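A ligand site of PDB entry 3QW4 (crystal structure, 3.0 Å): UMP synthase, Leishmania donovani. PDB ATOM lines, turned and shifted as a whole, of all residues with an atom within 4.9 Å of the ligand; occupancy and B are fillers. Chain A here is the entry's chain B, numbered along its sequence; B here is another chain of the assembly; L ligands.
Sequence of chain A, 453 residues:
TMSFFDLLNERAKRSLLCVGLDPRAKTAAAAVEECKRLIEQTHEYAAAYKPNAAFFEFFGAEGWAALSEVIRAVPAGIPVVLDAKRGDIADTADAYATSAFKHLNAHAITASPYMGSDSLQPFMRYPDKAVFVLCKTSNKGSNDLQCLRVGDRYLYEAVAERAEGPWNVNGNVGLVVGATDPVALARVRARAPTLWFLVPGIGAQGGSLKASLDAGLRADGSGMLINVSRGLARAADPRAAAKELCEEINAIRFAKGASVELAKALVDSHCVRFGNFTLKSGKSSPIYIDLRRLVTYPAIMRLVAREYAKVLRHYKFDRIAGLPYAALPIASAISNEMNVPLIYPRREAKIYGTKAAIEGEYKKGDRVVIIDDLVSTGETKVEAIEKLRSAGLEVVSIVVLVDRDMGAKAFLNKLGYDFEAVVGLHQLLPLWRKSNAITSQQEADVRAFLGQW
Asp 83 touches the ligand.
Lys 85 touches the ligand.
Thr 137 touches the ligand.
CG1 of Val 176 touches C3 of the ligand, at 3.8 Å.
CB of Pro 200 touches C1 of the ligand, at 3.5 Å.
O of Ile 202 touches O9 of the ligand (3.99 Å).
OD1 of Asn 227 touches O6 of the ligand (3.8 Å).
Val 228 touches the ligand (C to O9, 3.9 Å).
Ile 89 of chain B touches the ligand.
Hydrophobic or aromatic side chains within 4 Å of the ligand: Val 176, Pro 200 and Ile 89 of chain B.
The nearest printed residue that does not touch the ligand is Ala 204 (4.02 Å).
The side-chain carboxylate (OD2) of Asp 22 lies close to the backbone NH (N) of Asn 52, at 3.5 Å.
OD2 of Asp 88 of chain B is in salt-bridge range of NZ of Lys 85 (2.7 Å).
The side-chain hydroxyl (OG) of Ser 229 sits at hydrogen-bond distance from the side-chain carboxylate (OD1) of Asp 22.
The side-chain amide nitrogen (NE2) of Gln 205 lies within hydrogen-bond range of the side-chain hydroxyl (OG) of Ser 138, 2.8 Å away.
The side-chain amide oxygen of Asn 139 sits at hydrogen-bond distance from the side-chain hydroxyl of Thr 137 (2.8 Å).
The side-chain amino group of Lys 50 lies within salt-bridge range of the side-chain carboxylate of Asp 83, at 3.1 Å.
The side-chain amide oxygen of Asn 227 sits at hydrogen-bond distance from the side-chain amino group of Lys 50.
NZ of Lys 85 is in salt-bridge range of OD1 of Asp 83 (2.6 Å).
The side-chain amide nitrogen (ND2) of Asn 52 lies within hydrogen-bond range of an oxygen (O4) of the ligand (2.6 Å).
The side-chain carboxylate (OD1) of Asp 88 of chain B is in hydrogen-bond range of an oxygen (O3) of the ligand (2.6 Å).
N of Arg 230 lies within hydrogen-bond range of O9 of the ligand (3.3 Å).
NE of Arg 230 lies within salt-bridge range of O7 of the ligand (2.7 Å).
The backbone NH (N) of Ser 229 sits at hydrogen-bond distance from an oxygen (O9) of the ligand.
OG of Ser 229 lies within hydrogen-bond range of O7 of the ligand (2.8 Å).
OE1 of Gln 205 lies close to O1 of the ligand (3.0 Å).
The backbone NH (N) of Ser 138 lies within hydrogen-bond range of an oxygen (O2) of the ligand, 3.2 Å away.
The side-chain carboxylate (OD1) of Asp 22 is in hydrogen-bond range of an oxygen (O4) of the ligand, at 3.2 Å.
An oxygen (O5) of the ligand is in hydrogen-bond range of the side-chain amino group (NZ) of Lys 50 (3.3 Å).
The side-chain hydroxyl (OG1) of Thr 92 of chain B lies within hydrogen-bond range of an oxygen (O3) of the ligand (3.4 Å).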
ATOM      1  N   ASP A  22      10.761 -21.347  -9.842  1.00  0.00           N
ATOM      2  CA  ASP A  22      11.533 -22.483  -9.372  1.00  0.00           C
ATOM      3  C   ASP A  22      12.977 -22.027  -9.197  1.00  0.00           C
ATOM      4  O   ASP A  22      13.808 -22.238 -10.094  1.00  0.00           O
ATOM      5  CB  ASP A  22      11.528 -23.625 -10.400  1.00  0.00           C
ATOM      6  CG  ASP A  22      10.152 -23.915 -10.977  1.00  0.00           C
ATOM      7  OD1 ASP A  22      10.118 -24.581 -12.037  1.00  0.00           O
ATOM      8  OD2 ASP A  22       9.117 -23.509 -10.394  1.00  0.00           O
ATOM      9  N   LYS A  50       3.586 -19.223 -10.860  1.00  0.00           N
ATOM     10  CA  LYS A  50       3.573 -20.598 -10.395  1.00  0.00           C
ATOM     11  C   LYS A  50       4.883 -20.992  -9.708  1.00  0.00           C
ATOM     12  O   LYS A  50       5.834 -21.410 -10.384  1.00  0.00           O
ATOM     13  CB  LYS A  50       3.267 -21.530 -11.570  1.00  0.00           C
ATOM     14  CG  LYS A  50       2.785 -22.910 -11.194  1.00  0.00           C
ATOM     15  CD  LYS A  50       3.043 -23.866 -12.335  1.00  0.00           C
ATOM     16  CE  LYS A  50       4.481 -24.352 -12.317  1.00  0.00           C
ATOM     17  NZ  LYS A  50       4.647 -25.420 -13.319  1.00  0.00           N
ATOM     18  N   ASN A  52       6.979 -23.625  -7.654  1.00  0.00           N
ATOM     19  CA  ASN A  52       7.006 -25.055  -7.358  1.00  0.00           C
ATOM     20  C   ASN A  52       7.639 -25.332  -6.005  1.00  0.00           C
ATOM     21  O   ASN A  52       8.804 -25.004  -5.791  1.00  0.00           O
ATOM     22  CB  ASN A  52       7.715 -25.843  -8.456  1.00  0.00           C
ATOM     23  CG  ASN A  52       7.494 -27.339  -8.350  1.00  0.00           C
ATOM     24  OD1 ASN A  52       7.852 -27.973  -7.368  1.00  0.00           O
ATOM     25  ND2 ASN A  52       6.920 -27.914  -9.385  1.00  0.00           N
ATOM     26  N   PHE A  55      11.482 -26.541  -4.654  1.00  0.00           N
ATOM     27  CA  PHE A  55      12.685 -25.731  -4.633  1.00  0.00           C
ATOM     28  C   PHE A  55      12.747 -24.849  -3.420  1.00  0.00           C
ATOM     29  O   PHE A  55      13.826 -24.428  -3.003  1.00  0.00           O
ATOM     30  CB  PHE A  55      12.814 -24.920  -5.924  1.00  0.00           C
ATOM     31  CG  PHE A  55      12.757 -25.768  -7.160  1.00  0.00           C
ATOM     32  CD1 PHE A  55      11.539 -26.010  -7.807  1.00  0.00           C
ATOM     33  CD2 PHE A  55      13.920 -26.363  -7.658  1.00  0.00           C
ATOM     34  CE1 PHE A  55      11.474 -26.822  -8.939  1.00  0.00           C
ATOM     35  CE2 PHE A  55      13.875 -27.173  -8.792  1.00  0.00           C
ATOM     36  CZ  PHE A  55      12.646 -27.407  -9.441  1.00  0.00           C
ATOM     37  N   ASP A  83       2.319 -25.192  -7.227  1.00  0.00           N
ATOM     38  CA  ASP A  83       2.561 -26.476  -7.837  1.00  0.00           C
ATOM     39  C   ASP A  83       3.163 -27.373  -6.779  1.00  0.00           C
ATOM     40  O   ASP A  83       4.373 -27.342  -6.547  1.00  0.00           O
ATOM     41  CB  ASP A  83       3.463 -26.360  -9.045  1.00  0.00           C
ATOM     42  CG  ASP A  83       3.344 -27.560  -9.984  1.00  0.00           C
ATOM     43  OD1 ASP A  83       2.737 -28.575  -9.588  1.00  0.00           O
ATOM     44  OD2 ASP A  83       3.876 -27.496 -11.116  1.00  0.00           O
ATOM     45  N   LYS A  85       1.450 -30.657  -6.126  1.00  0.00           N
ATOM     46  CA  LYS A  85       0.964 -32.005  -6.416  1.00  0.00           C
ATOM     47  C   LYS A  85       0.520 -32.751  -5.163  1.00  0.00           C
ATOM     48  O   LYS A  85       1.119 -33.743  -4.767  1.00  0.00           O
ATOM     49  CB  LYS A  85       2.020 -32.803  -7.180  1.00  0.00           C
ATOM     50  CG  LYS A  85       2.206 -32.310  -8.576  1.00  0.00           C
ATOM     51  CD  LYS A  85       3.505 -32.754  -9.179  1.00  0.00           C
ATOM     52  CE  LYS A  85       3.773 -31.928 -10.418  1.00  0.00           C
ATOM     53  NZ  LYS A  85       4.289 -30.586 -10.064  1.00  0.00           N
ATOM     54  N   LEU A 134      -3.455 -33.441 -12.623  1.00  0.00           N
ATOM     55  CA  LEU A 134      -2.470 -33.927 -13.568  1.00  0.00           C
ATOM     56  C   LEU A 134      -3.131 -34.832 -14.599  1.00  0.00           C
ATOM     57  O   LEU A 134      -3.787 -35.800 -14.235  1.00  0.00           O
ATOM     58  CB  LEU A 134      -1.387 -34.702 -12.819  1.00  0.00           C
ATOM     59  CG  LEU A 134      -0.514 -33.896 -11.842  1.00  0.00           C
ATOM     60  CD1 LEU A 134       0.311 -34.779 -10.914  1.00  0.00           C
ATOM     61  CD2 LEU A 134       0.388 -32.923 -12.583  1.00  0.00           C
ATOM     62  N   THR A 137       1.281 -35.456 -18.525  1.00  0.00           N
ATOM     63  CA  THR A 137       2.416 -34.697 -18.047  1.00  0.00           C
ATOM     64  C   THR A 137       3.523 -34.525 -19.077  1.00  0.00           C
ATOM     65  O   THR A 137       3.655 -35.341 -19.985  1.00  0.00           O
ATOM     66  CB  THR A 137       2.972 -35.305 -16.757  1.00  0.00           C
ATOM     67  OG1 THR A 137       3.283 -36.694 -16.962  1.00  0.00           O
ATOM     68  CG2 THR A 137       1.947 -35.155 -15.630  1.00  0.00           C
ATOM     69  N   SER A 138       4.298 -33.465 -18.889  1.00  0.00           N
ATOM     70  CA  SER A 138       5.328 -33.041 -19.842  1.00  0.00           C
ATOM     71  C   SER A 138       6.439 -34.067 -20.088  1.00  0.00           C
ATOM     72  O   SER A 138       6.985 -34.128 -21.187  1.00  0.00           O
ATOM     73  CB  SER A 138       5.945 -31.731 -19.372  1.00  0.00           C
ATOM     74  OG  SER A 138       7.119 -31.438 -20.111  1.00  0.00           O
ATOM     75  N   ASN A 139       6.773 -34.838 -19.064  1.00  0.00           N
ATOM     76  CA  ASN A 139       7.847 -35.829 -19.136  1.00  0.00           C
ATOM     77  C   ASN A 139       7.549 -36.972 -20.095  1.00  0.00           C
ATOM     78  O   ASN A 139       6.400 -37.330 -20.278  1.00  0.00           O
ATOM     79  CB  ASN A 139       8.182 -36.384 -17.741  1.00  0.00           C
ATOM     80  CG  ASN A 139       6.953 -36.948 -17.023  1.00  0.00           C
ATOM     81  OD1 ASN A 139       6.005 -36.223 -16.718  1.00  0.00           O
ATOM     82  ND2 ASN A 139       6.980 -38.251 -16.730  1.00  0.00           N
ATOM     83  N   VAL A 176      -3.580 -30.250 -15.980  1.00  0.00           N
ATOM     84  CA  VAL A 176      -2.188 -30.052 -16.338  1.00  0.00           C
ATOM     85  C   VAL A 176      -1.942 -30.952 -17.529  1.00  0.00           C
ATOM     86  O   VAL A 176      -1.961 -32.170 -17.433  1.00  0.00           O
ATOM     87  CB  VAL A 176      -1.216 -30.438 -15.203  1.00  0.00           C
ATOM     88  CG1 VAL A 176       0.233 -30.205 -15.634  1.00  0.00           C
ATOM     89  CG2 VAL A 176      -1.509 -29.682 -13.920  1.00  0.00           C
ATOM     90  N   PRO A 200       2.828 -26.759 -19.055  1.00  0.00           N
ATOM     91  CA  PRO A 200       4.273 -26.694 -18.930  1.00  0.00           C
ATOM     92  C   PRO A 200       4.994 -27.378 -20.100  1.00  0.00           C
ATOM     93  O   PRO A 200       4.383 -28.165 -20.817  1.00  0.00           O
ATOM     94  CB  PRO A 200       4.548 -27.462 -17.631  1.00  0.00           C
ATOM     95  CG  PRO A 200       3.252 -28.215 -17.307  1.00  0.00           C
ATOM     96  CD  PRO A 200       2.273 -27.956 -18.405  1.00  0.00           C
ATOM     97  N   GLY A 201       6.271 -27.048 -20.287  1.00  0.00           N
ATOM     98  CA  GLY A 201       7.083 -27.654 -21.359  1.00  0.00           C
ATOM     99  C   GLY A 201       7.778 -26.716 -22.339  1.00  0.00           C
ATOM    100  O   GLY A 201       8.623 -27.149 -23.114  1.00  0.00           O
ATOM    101  N   ILE A 202       7.415 -25.433 -22.325  1.00  0.00           N
ATOM    102  CA  ILE A 202       8.066 -24.455 -23.175  1.00  0.00           C
ATOM    103  C   ILE A 202       9.407 -24.043 -22.574  1.00  0.00           C
ATOM    104  O   ILE A 202       9.493 -23.714 -21.397  1.00  0.00           O
ATOM    105  CB  ILE A 202       7.141 -23.221 -23.404  1.00  0.00           C
ATOM    106  CG1 ILE A 202       5.927 -23.612 -24.233  1.00  0.00           C
ATOM    107  CG2 ILE A 202       7.841 -22.101 -24.141  1.00  0.00           C
ATOM    108  CD1 ILE A 202       4.700 -23.913 -23.376  1.00  0.00           C
ATOM    109  N   ALA A 204      12.961 -24.963 -21.453  1.00  0.00           N
ATOM    110  CA  ALA A 204      13.878 -26.010 -20.992  1.00  0.00           C
ATOM    111  C   ALA A 204      13.583 -27.393 -21.572  1.00  0.00           C
ATOM    112  O   ALA A 204      14.498 -28.180 -21.860  1.00  0.00           O
ATOM    113  CB  ALA A 204      13.873 -26.059 -19.460  1.00  0.00           C
ATOM    114  N   GLN A 205      12.301 -27.701 -21.747  1.00  0.00           N
ATOM    115  CA  GLN A 205      11.888 -29.015 -22.209  1.00  0.00           C
ATOM    116  C   GLN A 205      11.605 -28.981 -23.709  1.00  0.00           C
ATOM    117  O   GLN A 205      11.268 -29.987 -24.326  1.00  0.00           O
ATOM    118  CB  GLN A 205      10.675 -29.497 -21.416  1.00  0.00           C
ATOM    119  CG  GLN A 205      10.878 -29.489 -19.889  1.00  0.00           C
ATOM    120  CD  GLN A 205       9.725 -30.143 -19.180  1.00  0.00           C
ATOM    121  OE1 GLN A 205       8.819 -29.466 -18.692  1.00  0.00           O
ATOM    122  NE2 GLN A 205       9.726 -31.483 -19.138  1.00  0.00           N
ATOM    123  N   ASN A 227       3.007 -22.055 -19.069  1.00  0.00           N
ATOM    124  CA  ASN A 227       4.017 -21.904 -18.030  1.00  0.00           C
ATOM    125  C   ASN A 227       5.475 -21.963 -18.536  1.00  0.00           C
ATOM    126  O   ASN A 227       5.864 -22.902 -19.281  1.00  0.00           O
ATOM    127  CB  ASN A 227       3.803 -22.944 -16.933  1.00  0.00           C
ATOM    128  CG  ASN A 227       4.913 -22.909 -15.896  1.00  0.00           C
ATOM    129  OD1 ASN A 227       5.815 -23.772 -15.908  1.00  0.00           O
ATOM    130  ND2 ASN A 227       4.894 -21.899 -15.021  1.00  0.00           N
ATOM    131  N   VAL A 228       6.257 -20.966 -18.134  1.00  0.00           N
ATOM    132  CA  VAL A 228       7.673 -20.938 -18.409  1.00  0.00           C
ATOM    133  C   VAL A 228       8.392 -20.576 -17.121  1.00  0.00           C
ATOM    134  O   VAL A 228       8.090 -19.550 -16.494  1.00  0.00           O
ATOM    135  CB  VAL A 228       8.061 -19.904 -19.493  1.00  0.00           C
ATOM    136  CG1 VAL A 228       9.514 -20.060 -19.878  1.00  0.00           C
ATOM    137  CG2 VAL A 228       7.206 -20.069 -20.719  1.00  0.00           C
ATOM    138  N   SER A 229       9.338 -21.408 -16.699  1.00  0.00           N
ATOM    139  CA  SER A 229      10.067 -21.161 -15.466  1.00  0.00           C
ATOM    140  C   SER A 229      11.564 -20.908 -15.707  1.00  0.00           C
ATOM    141  O   SER A 229      12.038 -19.794 -15.533  1.00  0.00           O
ATOM    142  CB  SER A 229       9.797 -22.263 -14.437  1.00  0.00           C
ATOM    143  OG  SER A 229      10.590 -23.407 -14.696  1.00  0.00           O
ATOM    144  N   ARG A 230      12.306 -21.938 -16.109  1.00  0.00           N
ATOM    145  CA  ARG A 230      13.745 -21.788 -16.379  1.00  0.00           C
ATOM    146  C   ARG A 230      14.011 -20.957 -17.630  1.00  0.00           C
ATOM    147  O   ARG A 230      15.033 -20.274 -17.722  1.00  0.00           O
ATOM    148  CB  ARG A 230      14.435 -23.160 -16.488  1.00  0.00           C
ATOM    149  CG  ARG A 230      14.717 -23.844 -15.167  1.00  0.00           C
ATOM    150  CD  ARG A 230      15.232 -25.266 -15.385  1.00  0.00           C
ATOM    151  NE  ARG A 230      14.204 -26.136 -15.944  1.00  0.00           N
ATOM    152  CZ  ARG A 230      14.330 -27.459 -16.138  1.00  0.00           C
ATOM    153  NH1 ARG A 230      15.458 -28.079 -15.817  1.00  0.00           N
ATOM    154  NH2 ARG A 230      13.318 -28.149 -16.647  1.00  0.00           N
ATOM    155  N   GLY A 231      13.095 -20.995 -18.595  1.00  0.00           N
ATOM    156  CA  GLY A 231      13.217 -20.199 -19.804  1.00  0.00           C
ATOM    157  C   GLY A 231      13.272 -18.703 -19.546  1.00  0.00           C
ATOM    158  O   GLY A 231      13.757 -17.933 -20.384  1.00  0.00           O
ATOM    159  N   ASP B  88       7.161 -35.828  -9.392  1.00  0.00           N
ATOM    160  CA  ASP B  88       7.231 -34.708 -10.328  1.00  0.00           C
ATOM    161  C   ASP B  88       8.248 -35.054 -11.403  1.00  0.00           C
ATOM    162  O   ASP B  88       8.818 -36.143 -11.365  1.00  0.00           O
ATOM    163  CB  ASP B  88       7.658 -33.435  -9.595  1.00  0.00           C
ATOM    164  CG  ASP B  88       7.196 -32.160 -10.295  1.00  0.00           C
ATOM    165  OD1 ASP B  88       7.103 -32.132 -11.549  1.00  0.00           O
ATOM    166  OD2 ASP B  88       6.919 -31.178  -9.591  1.00  0.00           O
ATOM    167  N   ILE B  89       8.462 -34.145 -12.355  1.00  0.00           N
ATOM    168  CA  ILE B  89       9.473 -34.342 -13.398  1.00  0.00           C
ATOM    169  C   ILE B  89      10.883 -34.490 -12.804  1.00  0.00           C
ATOM    170  O   ILE B  89      11.226 -33.806 -11.833  1.00  0.00           O
ATOM    171  CB  ILE B  89       9.459 -33.247 -14.496  1.00  0.00           C
ATOM    172  CG1 ILE B  89       9.960 -31.900 -13.972  1.00  0.00           C
ATOM    173  CG2 ILE B  89       8.068 -33.114 -15.109  1.00  0.00           C
ATOM    174  CD1 ILE B  89      10.761 -31.113 -14.996  1.00  0.00           C
ATOM    175  N   THR B  92      12.728 -31.771 -11.012  1.00  0.00           N
ATOM    176  CA  THR B  92      12.061 -31.257  -9.829  1.00  0.00           C
ATOM    177  C   THR B  92      12.101 -32.322  -8.745  1.00  0.00           C
ATOM    178  O   THR B  92      12.289 -32.014  -7.573  1.00  0.00           O
ATOM    179  CB  THR B  92      10.622 -30.798 -10.136  1.00  0.00           C
ATOM    180  OG1 THR B  92      10.643 -29.849 -11.207  1.00  0.00           O
ATOM    181  CG2 THR B  92       9.979 -30.146  -8.932  1.00  0.00           C
ATOM    182  N   MET B 115       3.092 -40.198 -12.837  1.00  0.00           N
ATOM    183  CA  MET B 115       3.963 -39.551 -13.797  1.00  0.00           C
ATOM    184  C   MET B 115       5.011 -40.490 -14.412  1.00  0.00           C
ATOM    185  O   MET B 115       5.980 -40.039 -15.023  1.00  0.00           O
ATOM    186  CB  MET B 115       4.583 -38.280 -13.196  1.00  0.00           C
ATOM    187  CG  MET B 115       3.581 -37.125 -13.107  1.00  0.00           C
ATOM    188  SD  MET B 115       4.229 -35.612 -12.404  1.00  0.00           S
ATOM    189  CE  MET B 115       5.263 -35.029 -13.726  1.00  0.00           C
HETATM  190  N1  LIG L   1       5.665 -29.369 -14.410  1.00  0.00           N
HETATM  191  C1  LIG L   1       6.051 -29.931 -15.658  1.00  0.00           C
HETATM  192  N2  LIG L   1       5.264 -30.926 -16.233  1.00  0.00           N
HETATM  193  C2  LIG L   1       4.116 -31.368 -15.592  1.00  0.00           C
HETATM  194  C3  LIG L   1       3.738 -30.822 -14.361  1.00  0.00           C
HETATM  195  C4  LIG L   1       4.507 -29.825 -13.774  1.00  0.00           C
HETATM  196  O1  LIG L   1       7.049 -29.582 -16.267  1.00  0.00           O
HETATM  197  O2  LIG L   1       3.419 -32.234 -16.108  1.00  0.00           O
HETATM  198  C5  LIG L   1       6.455 -28.302 -13.722  1.00  0.00           C
HETATM  199  C6  LIG L   1       7.683 -28.887 -13.062  1.00  0.00           C
HETATM  200  O3  LIG L   1       7.339 -29.548 -11.843  1.00  0.00           O
HETATM  201  C7  LIG L   1       8.475 -27.615 -12.794  1.00  0.00           C
HETATM  202  C8  LIG L   1       7.979 -26.615 -13.839  1.00  0.00           C
HETATM  203  O4  LIG L   1       8.183 -27.119 -11.491  1.00  0.00           O
HETATM  204  O5  LIG L   1       7.010 -27.313 -14.597  1.00  0.00           O
HETATM  205  C9  LIG L   1       9.221 -26.487 -14.677  1.00  0.00           C
HETATM  206  O6  LIG L   1       9.007 -25.744 -15.857  1.00  0.00           O
HETATM  207  P1  LIG L   1      10.273 -25.518 -16.820  1.00  0.00           P
HETATM  208  O7  LIG L   1      11.551 -25.644 -16.088  1.00  0.00           O
HETATM  209  O8  LIG L   1      10.136 -26.549 -18.065  1.00  0.00           O
HETATM  210  O9  LIG L   1      10.118 -24.038 -17.473  1.00  0.00           O
